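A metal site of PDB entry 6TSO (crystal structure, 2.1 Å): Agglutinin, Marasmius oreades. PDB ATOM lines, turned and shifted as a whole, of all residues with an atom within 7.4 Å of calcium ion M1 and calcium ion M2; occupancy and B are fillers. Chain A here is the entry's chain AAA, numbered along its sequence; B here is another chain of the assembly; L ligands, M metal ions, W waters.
Five residues have an atom within 4 Å of calcium ion M1: Gln 211, Asp 214, Asp 216, Asp 217 and Asp 183 of chain B.
The nearest printed residue that does not touch calcium ion M2 is Gln 211 (4.9 Å).
OD1 of Asp 214 is bound to calcium ion M1 (2.3 Å). Calcium ion M1 is bound by OD2 of Asp 216, 2.3 Å away. Calcium ion M1 is bound by OD2 of Asp 217. Water W2 binds calcium ion M1 (2.4 Å). O of Gln 211 binds calcium ion M1, 2.5 Å away. Calcium ion M1 is bound by OD2 of Asp 183 of chain B, at 2.5 Å. OD1 of Asp 183 of chain B binds calcium ion M1 (2.6 Å).
Calcium ion M2 is bound by OD2 of Asp 214 (2.3 Å), O of Leu 182 of chain B (2.3 Å), OD1 of Asp 216 (2.4 Å), O1 of the ligand (2.4 Å), OD1 of Asp 183 of chain B (2.4 Å) and water W1 (2.5 Å). Calcium ion M2 has six donor atoms within binding distance.
The backbone carbonyl oxygen of Arg 209 lies within hydrogen-bond range of the backbone NH of Asp 214 (3.4 Å). The chain-end carboxylate (OXT) of Tyr 293 of chain B sits at hydrogen-bond distance from the backbone NH (N) of Leu 182 of chain B, 2.7 Å away. N of Asp 183 of chain B sits at hydrogen-bond distance from OH of Tyr 186 of chain B (2.9 Å). N of Gly 184 of chain B lies within hydrogen-bond range of OE1 of Gln 211 (3.1 Å).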
ATOM      1  N   TRP A 208      23.439  -5.578  -4.274  1.00  0.00           N
ATOM      2  CA  TRP A 208      22.285  -5.298  -3.390  1.00  0.00           C
ATOM      3  C   TRP A 208      22.720  -4.246  -2.374  1.00  0.00           C
ATOM      4  O   TRP A 208      23.707  -4.466  -1.627  1.00  0.00           O
ATOM      5  CB  TRP A 208      21.791  -6.553  -2.696  1.00  0.00           C
ATOM      6  CG  TRP A 208      20.551  -6.303  -1.887  1.00  0.00           C
ATOM      7  CD1 TRP A 208      19.265  -6.537  -2.267  1.00  0.00           C
ATOM      8  CD2 TRP A 208      20.489  -5.811  -0.540  1.00  0.00           C
ATOM      9  NE1 TRP A 208      18.401  -6.214  -1.254  1.00  0.00           N
ATOM     10  CE2 TRP A 208      19.127  -5.753  -0.190  1.00  0.00           C
ATOM     11  CE3 TRP A 208      21.452  -5.406   0.401  1.00  0.00           C
ATOM     12  CZ2 TRP A 208      18.700  -5.328   1.073  1.00  0.00           C
ATOM     13  CZ3 TRP A 208      21.033  -4.972   1.635  1.00  0.00           C
ATOM     14  CH2 TRP A 208      19.672  -4.944   1.974  1.00  0.00           C
ATOM     15  N   ARG A 209      21.986  -3.148  -2.352  1.00  0.00           N
ATOM     16  CA  ARG A 209      22.146  -2.060  -1.372  1.00  0.00           C
ATOM     17  C   ARG A 209      20.751  -1.744  -0.854  1.00  0.00           C
ATOM     18  O   ARG A 209      19.845  -1.529  -1.692  1.00  0.00           O
ATOM     19  CB  ARG A 209      22.828  -0.869  -2.058  1.00  0.00           C
ATOM     20  CG  ARG A 209      24.219  -1.157  -2.594  1.00  0.00           C
ATOM     21  CD  ARG A 209      24.799  -0.031  -3.452  1.00  0.00           C
ATOM     22  NE  ARG A 209      24.756   1.199  -2.688  1.00  0.00           N
ATOM     23  CZ  ARG A 209      24.892   2.433  -3.171  1.00  0.00           C
ATOM     24  NH1 ARG A 209      25.117   2.664  -4.453  1.00  0.00           N
ATOM     25  NH2 ARG A 209      24.836   3.438  -2.302  1.00  0.00           N
ATOM     26  N   GLU A 210      20.609  -1.700   0.471  1.00  0.00           N
ATOM     27  CA  GLU A 210      19.353  -1.383   1.185  1.00  0.00           C
ATOM     28  C   GLU A 210      18.666  -0.152   0.566  1.00  0.00           C
ATOM     29  O   GLU A 210      19.263   0.950   0.603  1.00  0.00           O
ATOM     30  CB  GLU A 210      19.655  -1.129   2.656  1.00  0.00           C
ATOM     31  CG  GLU A 210      18.438  -1.322   3.545  1.00  0.00           C
ATOM     32  CD  GLU A 210      18.736  -1.040   4.998  1.00  0.00           C
ATOM     33  OE1 GLU A 210      19.908  -1.174   5.393  1.00  0.00           O
ATOM     34  OE2 GLU A 210      17.793  -0.670   5.728  1.00  0.00           O
ATOM     35  N   GLN A 211      17.459  -0.356   0.037  1.00  0.00           N
ATOM     36  CA  GLN A 211      16.531   0.651  -0.576  1.00  0.00           C
ATOM     37  C   GLN A 211      17.158   1.276  -1.849  1.00  0.00           C
ATOM     38  O   GLN A 211      16.421   1.410  -2.847  1.00  0.00           O
ATOM     39  CB  GLN A 211      16.161   1.710   0.467  1.00  0.00           C
ATOM     40  CG  GLN A 211      15.313   1.153   1.621  1.00  0.00           C
ATOM     41  CD  GLN A 211      14.507   2.216   2.345  1.00  0.00           C
ATOM     42  OE1 GLN A 211      13.962   3.133   1.735  1.00  0.00           O
ATOM     43  NE2 GLN A 211      14.407   2.096   3.657  1.00  0.00           N
ATOM     44  N   ILE A 212      18.461   1.598  -1.887  1.00  0.00           N
ATOM     45  CA  ILE A 212      19.030   2.416  -3.003  1.00  0.00           C
ATOM     46  C   ILE A 212      19.191   1.557  -4.268  1.00  0.00           C
ATOM     47  O   ILE A 212      19.063   2.102  -5.384  1.00  0.00           O
ATOM     48  CB  ILE A 212      20.364   3.063  -2.567  1.00  0.00           C
ATOM     49  CG1 ILE A 212      20.768   4.136  -3.579  1.00  0.00           C
ATOM     50  CG2 ILE A 212      21.468   2.036  -2.352  1.00  0.00           C
ATOM     51  CD1 ILE A 212      19.773   5.235  -3.697  1.00  0.00           C
ATOM     52  N   TYR A 213      19.442   0.262  -4.092  1.00  0.00           N
ATOM     53  CA  TYR A 213      19.500  -0.727  -5.207  1.00  0.00           C
ATOM     54  C   TYR A 213      19.227  -2.114  -4.634  1.00  0.00           C
ATOM     55  O   TYR A 213      20.150  -2.966  -4.407  1.00  0.00           O
ATOM     56  CB  TYR A 213      20.839  -0.675  -5.929  1.00  0.00           C
ATOM     57  CG  TYR A 213      20.650  -0.830  -7.402  1.00  0.00           C
ATOM     58  CD1 TYR A 213      20.082   0.187  -8.132  1.00  0.00           C
ATOM     59  CD2 TYR A 213      20.938  -2.015  -8.063  1.00  0.00           C
ATOM     60  CE1 TYR A 213      19.830   0.064  -9.487  1.00  0.00           C
ATOM     61  CE2 TYR A 213      20.698  -2.150  -9.422  1.00  0.00           C
ATOM     62  CZ  TYR A 213      20.151  -1.106 -10.141  1.00  0.00           C
ATOM     63  OH  TYR A 213      19.909  -1.168 -11.494  1.00  0.00           O
ATOM     64  N   ASP A 214      17.957  -2.342  -4.365  1.00  0.00           N
ATOM     65  CA  ASP A 214      17.515  -3.616  -3.738  1.00  0.00           C
ATOM     66  C   ASP A 214      16.634  -4.302  -4.781  1.00  0.00           C
ATOM     67  O   ASP A 214      16.731  -3.938  -5.960  1.00  0.00           O
ATOM     68  CB  ASP A 214      16.902  -3.283  -2.387  1.00  0.00           C
ATOM     69  CG  ASP A 214      15.557  -2.548  -2.416  1.00  0.00           C
ATOM     70  OD1 ASP A 214      15.380  -1.601  -3.235  1.00  0.00           O
ATOM     71  OD2 ASP A 214      14.741  -2.872  -1.558  1.00  0.00           O
ATOM     72  N   CYS A 215      15.841  -5.300  -4.376  1.00  0.00           N
ATOM     73  CA  CYS A 215      15.175  -6.252  -5.309  1.00  0.00           C
ATOM     74  C   CYS A 215      14.268  -5.482  -6.291  1.00  0.00           C
ATOM     75  O   CYS A 215      14.280  -5.844  -7.514  1.00  0.00           O
ATOM     76  CB  CYS A 215      14.369  -7.303  -4.532  1.00  0.00           C
ATOM     77  SG  CYS A 215      13.387  -6.650  -3.165  1.00  0.00           S
ATOM     78  N   ASP A 216      13.488  -4.492  -5.850  1.00  0.00           N
ATOM     79  CA  ASP A 216      12.639  -3.714  -6.804  1.00  0.00           C
ATOM     80  C   ASP A 216      13.515  -3.055  -7.898  1.00  0.00           C
ATOM     81  O   ASP A 216      13.101  -3.030  -9.050  1.00  0.00           O
ATOM     82  CB  ASP A 216      11.802  -2.630  -6.132  1.00  0.00           C
ATOM     83  CG  ASP A 216      12.537  -1.826  -5.078  1.00  0.00           C
ATOM     84  OD1 ASP A 216      12.731  -2.348  -3.955  1.00  0.00           O
ATOM     85  OD2 ASP A 216      12.895  -0.666  -5.370  1.00  0.00           O
ATOM     86  N   ASP A 217      14.652  -2.478  -7.527  1.00  0.00           N
ATOM     87  CA  ASP A 217      15.558  -1.839  -8.522  1.00  0.00           C
ATOM     88  C   ASP A 217      16.061  -2.901  -9.523  1.00  0.00           C
ATOM     89  O   ASP A 217      16.030  -2.612 -10.744  1.00  0.00           O
ATOM     90  CB  ASP A 217      16.706  -1.127  -7.806  1.00  0.00           C
ATOM     91  CG  ASP A 217      16.204   0.005  -6.909  1.00  0.00           C
ATOM     92  OD1 ASP A 217      15.816   1.048  -7.465  1.00  0.00           O
ATOM     93  OD2 ASP A 217      16.169  -0.175  -5.681  1.00  0.00           O
ATOM     94  N   PHE A 218      16.443  -4.100  -9.076  1.00  0.00           N
ATOM     95  CA  PHE A 218      16.946  -5.146 -10.001  1.00  0.00           C
ATOM     96  C   PHE A 218      15.815  -5.590 -10.955  1.00  0.00           C
ATOM     97  O   PHE A 218      16.095  -5.759 -12.169  1.00  0.00           O
ATOM     98  CB  PHE A 218      17.523  -6.357  -9.273  1.00  0.00           C
ATOM     99  CG  PHE A 218      18.901  -6.212  -8.673  1.00  0.00           C
ATOM    100  CD1 PHE A 218      19.086  -5.570  -7.450  1.00  0.00           C
ATOM    101  CD2 PHE A 218      19.993  -6.819  -9.250  1.00  0.00           C
ATOM    102  CE1 PHE A 218      20.335  -5.506  -6.851  1.00  0.00           C
ATOM    103  CE2 PHE A 218      21.256  -6.723  -8.677  1.00  0.00           C
ATOM    104  CZ  PHE A 218      21.422  -6.079  -7.470  1.00  0.00           C
ATOM    105  N   ALA A 256       8.571  -9.254   1.821  1.00  0.00           N
ATOM    106  CA  ALA A 256       8.236  -8.999   0.399  1.00  0.00           C
ATOM    107  C   ALA A 256       9.524  -9.006  -0.433  1.00  0.00           C
ATOM    108  O   ALA A 256      10.595  -8.624   0.063  1.00  0.00           O
ATOM    109  CB  ALA A 256       7.475  -7.707   0.267  1.00  0.00           C
ATOM    110  N   ALA A 258      10.854  -8.644  -4.835  1.00  0.00           N
ATOM    111  CA  ALA A 258      10.605  -8.295  -6.246  1.00  0.00           C
ATOM    112  C   ALA A 258      11.506  -9.166  -7.133  1.00  0.00           C
ATOM    113  O   ALA A 258      12.703  -9.433  -6.771  1.00  0.00           O
ATOM    114  CB  ALA A 258      10.840  -6.814  -6.479  1.00  0.00           C
ATOM    115  N   ILE B 181       4.079   0.054  -3.072  1.00  0.00           N
ATOM    116  CA  ILE B 181       5.157   0.799  -2.368  1.00  0.00           C
ATOM    117  C   ILE B 181       6.396  -0.080  -2.461  1.00  0.00           C
ATOM    118  O   ILE B 181       6.288  -1.260  -2.131  1.00  0.00           O
ATOM    119  CB  ILE B 181       4.791   1.121  -0.909  1.00  0.00           C
ATOM    120  CG1 ILE B 181       3.764   2.240  -0.804  1.00  0.00           C
ATOM    121  CG2 ILE B 181       6.045   1.424  -0.094  1.00  0.00           C
ATOM    122  CD1 ILE B 181       2.359   1.853  -1.196  1.00  0.00           C
ATOM    123  N   LEU B 182       7.536   0.462  -2.900  1.00  0.00           N
ATOM    124  CA  LEU B 182       8.733  -0.395  -3.140  1.00  0.00           C
ATOM    125  C   LEU B 182       9.744  -0.178  -2.024  1.00  0.00           C
ATOM    126  O   LEU B 182      10.432  -1.133  -1.700  1.00  0.00           O
ATOM    127  CB  LEU B 182       9.338  -0.025  -4.510  1.00  0.00           C
ATOM    128  CG  LEU B 182       8.375  -0.261  -5.677  1.00  0.00           C
ATOM    129  CD1 LEU B 182       9.016   0.126  -7.011  1.00  0.00           C
ATOM    130  CD2 LEU B 182       7.913  -1.701  -5.707  1.00  0.00           C
ATOM    131  N   ASP B 183       9.789   1.018  -1.444  1.00  0.00           N
ATOM    132  CA  ASP B 183      10.822   1.455  -0.461  1.00  0.00           C
ATOM    133  C   ASP B 183      10.152   2.227   0.694  1.00  0.00           C
ATOM    134  O   ASP B 183       8.905   2.404   0.679  1.00  0.00           O
ATOM    135  CB  ASP B 183      11.906   2.245  -1.181  1.00  0.00           C
ATOM    136  CG  ASP B 183      12.669   1.447  -2.225  1.00  0.00           C
ATOM    137  OD1 ASP B 183      13.219   0.366  -1.846  1.00  0.00           O
ATOM    138  OD2 ASP B 183      12.656   1.857  -3.423  1.00  0.00           O
ATOM    139  N   GLY B 184      10.945   2.657   1.670  1.00  0.00           N
ATOM    140  CA  GLY B 184      10.480   3.335   2.900  1.00  0.00           C
ATOM    141  C   GLY B 184      10.774   4.830   2.960  1.00  0.00           C
ATOM    142  O   GLY B 184       9.998   5.528   3.601  1.00  0.00           O
ATOM    143  N   TYR B 186      12.524   8.282   0.632  1.00  0.00           N
ATOM    144  CA  TYR B 186      12.710   8.741  -0.764  1.00  0.00           C
ATOM    145  C   TYR B 186      13.284  10.154  -0.820  1.00  0.00           C
ATOM    146  O   TYR B 186      12.622  11.064  -0.336  1.00  0.00           O
ATOM    147  CB  TYR B 186      11.394   8.716  -1.510  1.00  0.00           C
ATOM    148  CG  TYR B 186      10.730   7.371  -1.633  1.00  0.00           C
ATOM    149  CD1 TYR B 186      11.028   6.534  -2.697  1.00  0.00           C
ATOM    150  CD2 TYR B 186       9.797   6.926  -0.699  1.00  0.00           C
ATOM    151  CE1 TYR B 186      10.422   5.297  -2.837  1.00  0.00           C
ATOM    152  CE2 TYR B 186       9.193   5.683  -0.816  1.00  0.00           C
ATOM    153  CZ  TYR B 186       9.487   4.888  -1.914  1.00  0.00           C
ATOM    154  OH  TYR B 186       8.904   3.671  -2.068  1.00  0.00           O
ATOM    155  N   LYS B 223      11.709   5.393 -14.712  1.00  0.00           N
ATOM    156  CA  LYS B 223      11.922   4.883 -13.334  1.00  0.00           C
ATOM    157  C   LYS B 223      13.271   4.144 -13.205  1.00  0.00           C
ATOM    158  O   LYS B 223      13.918   4.288 -12.149  1.00  0.00           O
ATOM    159  CB  LYS B 223      10.843   3.890 -12.910  1.00  0.00           C
ATOM    160  CG  LYS B 223      11.055   3.424 -11.490  1.00  0.00           C
ATOM    161  CD  LYS B 223       9.781   3.002 -10.803  1.00  0.00           C
ATOM    162  CE  LYS B 223      10.056   2.506  -9.407  1.00  0.00           C
ATOM    163  NZ  LYS B 223      10.742   3.547  -8.605  1.00  0.00           N
ATOM    164  N   GLY B 227      16.486   5.086 -10.657  1.00  0.00           N
ATOM    165  CA  GLY B 227      17.074   4.049  -9.777  1.00  0.00           C
ATOM    166  C   GLY B 227      18.572   3.887 -10.058  1.00  0.00           C
ATOM    167  O   GLY B 227      19.367   3.838  -9.113  1.00  0.00           O
ATOM    168  N   PHE B 239      17.941   4.387   1.715  1.00  0.00           N
ATOM    169  CA  PHE B 239      16.957   5.324   1.121  1.00  0.00           C
ATOM    170  C   PHE B 239      16.855   4.986  -0.351  1.00  0.00           C
ATOM    171  O   PHE B 239      17.787   4.378  -0.911  1.00  0.00           O
ATOM    172  CB  PHE B 239      17.363   6.791   1.306  1.00  0.00           C
ATOM    173  CG  PHE B 239      18.612   7.169   0.550  1.00  0.00           C
ATOM    174  CD1 PHE B 239      19.848   6.724   0.980  1.00  0.00           C
ATOM    175  CD2 PHE B 239      18.546   7.961  -0.580  1.00  0.00           C
ATOM    176  CE1 PHE B 239      21.004   7.053   0.289  1.00  0.00           C
ATOM    177  CE2 PHE B 239      19.699   8.266  -1.290  1.00  0.00           C
ATOM    178  CZ  PHE B 239      20.923   7.803  -0.868  1.00  0.00           C
ATOM    179  N   ALA B 240      15.796   5.483  -0.978  1.00  0.00           N
ATOM    180  CA  ALA B 240      15.580   5.394  -2.431  1.00  0.00           C
ATOM    181  C   ALA B 240      15.404   6.806  -3.008  1.00  0.00           C
ATOM    182  O   ALA B 240      15.357   7.760  -2.238  1.00  0.00           O
ATOM    183  CB  ALA B 240      14.394   4.540  -2.704  1.00  0.00           C
ATOM    184  N   ILE B 241      15.347   6.919  -4.342  1.00  0.00           N
ATOM    185  CA  ILE B 241      15.063   8.185  -5.069  1.00  0.00           C
ATOM    186  C   ILE B 241      13.607   8.149  -5.500  1.00  0.00           C
ATOM    187  O   ILE B 241      13.184   7.176  -6.102  1.00  0.00           O
ATOM    188  CB  ILE B 241      15.983   8.350  -6.281  1.00  0.00           C
ATOM    189  CG1 ILE B 241      17.445   8.073  -5.913  1.00  0.00           C
ATOM    190  CG2 ILE B 241      15.787   9.727  -6.891  1.00  0.00           C
ATOM    191  CD1 ILE B 241      17.987   8.856  -4.730  1.00  0.00           C
ATOM    192  N   TYR B 293       6.133   3.036  -6.937  1.00  0.00           N
ATOM    193  CA  TYR B 293       7.105   4.035  -6.430  1.00  0.00           C
ATOM    194  C   TYR B 293       7.857   3.407  -5.257  1.00  0.00           C
ATOM    195  O   TYR B 293       9.049   3.657  -5.087  1.00  0.00           O
ATOM    196  CB  TYR B 293       6.386   5.329  -6.027  1.00  0.00           C
ATOM    197  CG  TYR B 293       5.259   5.218  -5.033  1.00  0.00           C
ATOM    198  CD1 TYR B 293       3.945   5.064  -5.458  1.00  0.00           C
ATOM    199  CD2 TYR B 293       5.478   5.334  -3.678  1.00  0.00           C
ATOM    200  CE1 TYR B 293       2.903   4.986  -4.554  1.00  0.00           C
ATOM    201  CE2 TYR B 293       4.452   5.267  -2.760  1.00  0.00           C
ATOM    202  CZ  TYR B 293       3.155   5.109  -3.199  1.00  0.00           C
ATOM    203  OH  TYR B 293       2.129   5.056  -2.298  1.00  0.00           O
ATOM    204  OXT TYR B 293       7.281   2.614  -4.493  1.00  0.00           O
HETATM  205  C1  LIG L   1      10.527  -4.980  -1.507  1.00  0.00           C
HETATM  206  O1  LIG L   1      11.693  -4.213  -1.362  1.00  0.00           O
HETATM  207  C2  LIG L   1       9.648  -4.459  -2.570  1.00  0.00           C
HETATM  208  O2  LIG L   1       8.811  -5.449  -3.099  1.00  0.00           O
HETATM  209 CA    CA M   1      14.537   0.352  -4.074  1.00  0.00          CA
HETATM  210 CA    CA M   2      12.595  -1.986  -1.627  1.00  0.00          CA
HETATM  211 CD    CD M   3      14.217  -8.485  -1.617  1.00  0.00          CD
HETATM  212  O   HOH W   1      12.653  -1.560   0.854  1.00  0.00           O
HETATM  213  O   HOH W   2      14.612   2.160  -5.708  1.00  0.00           O
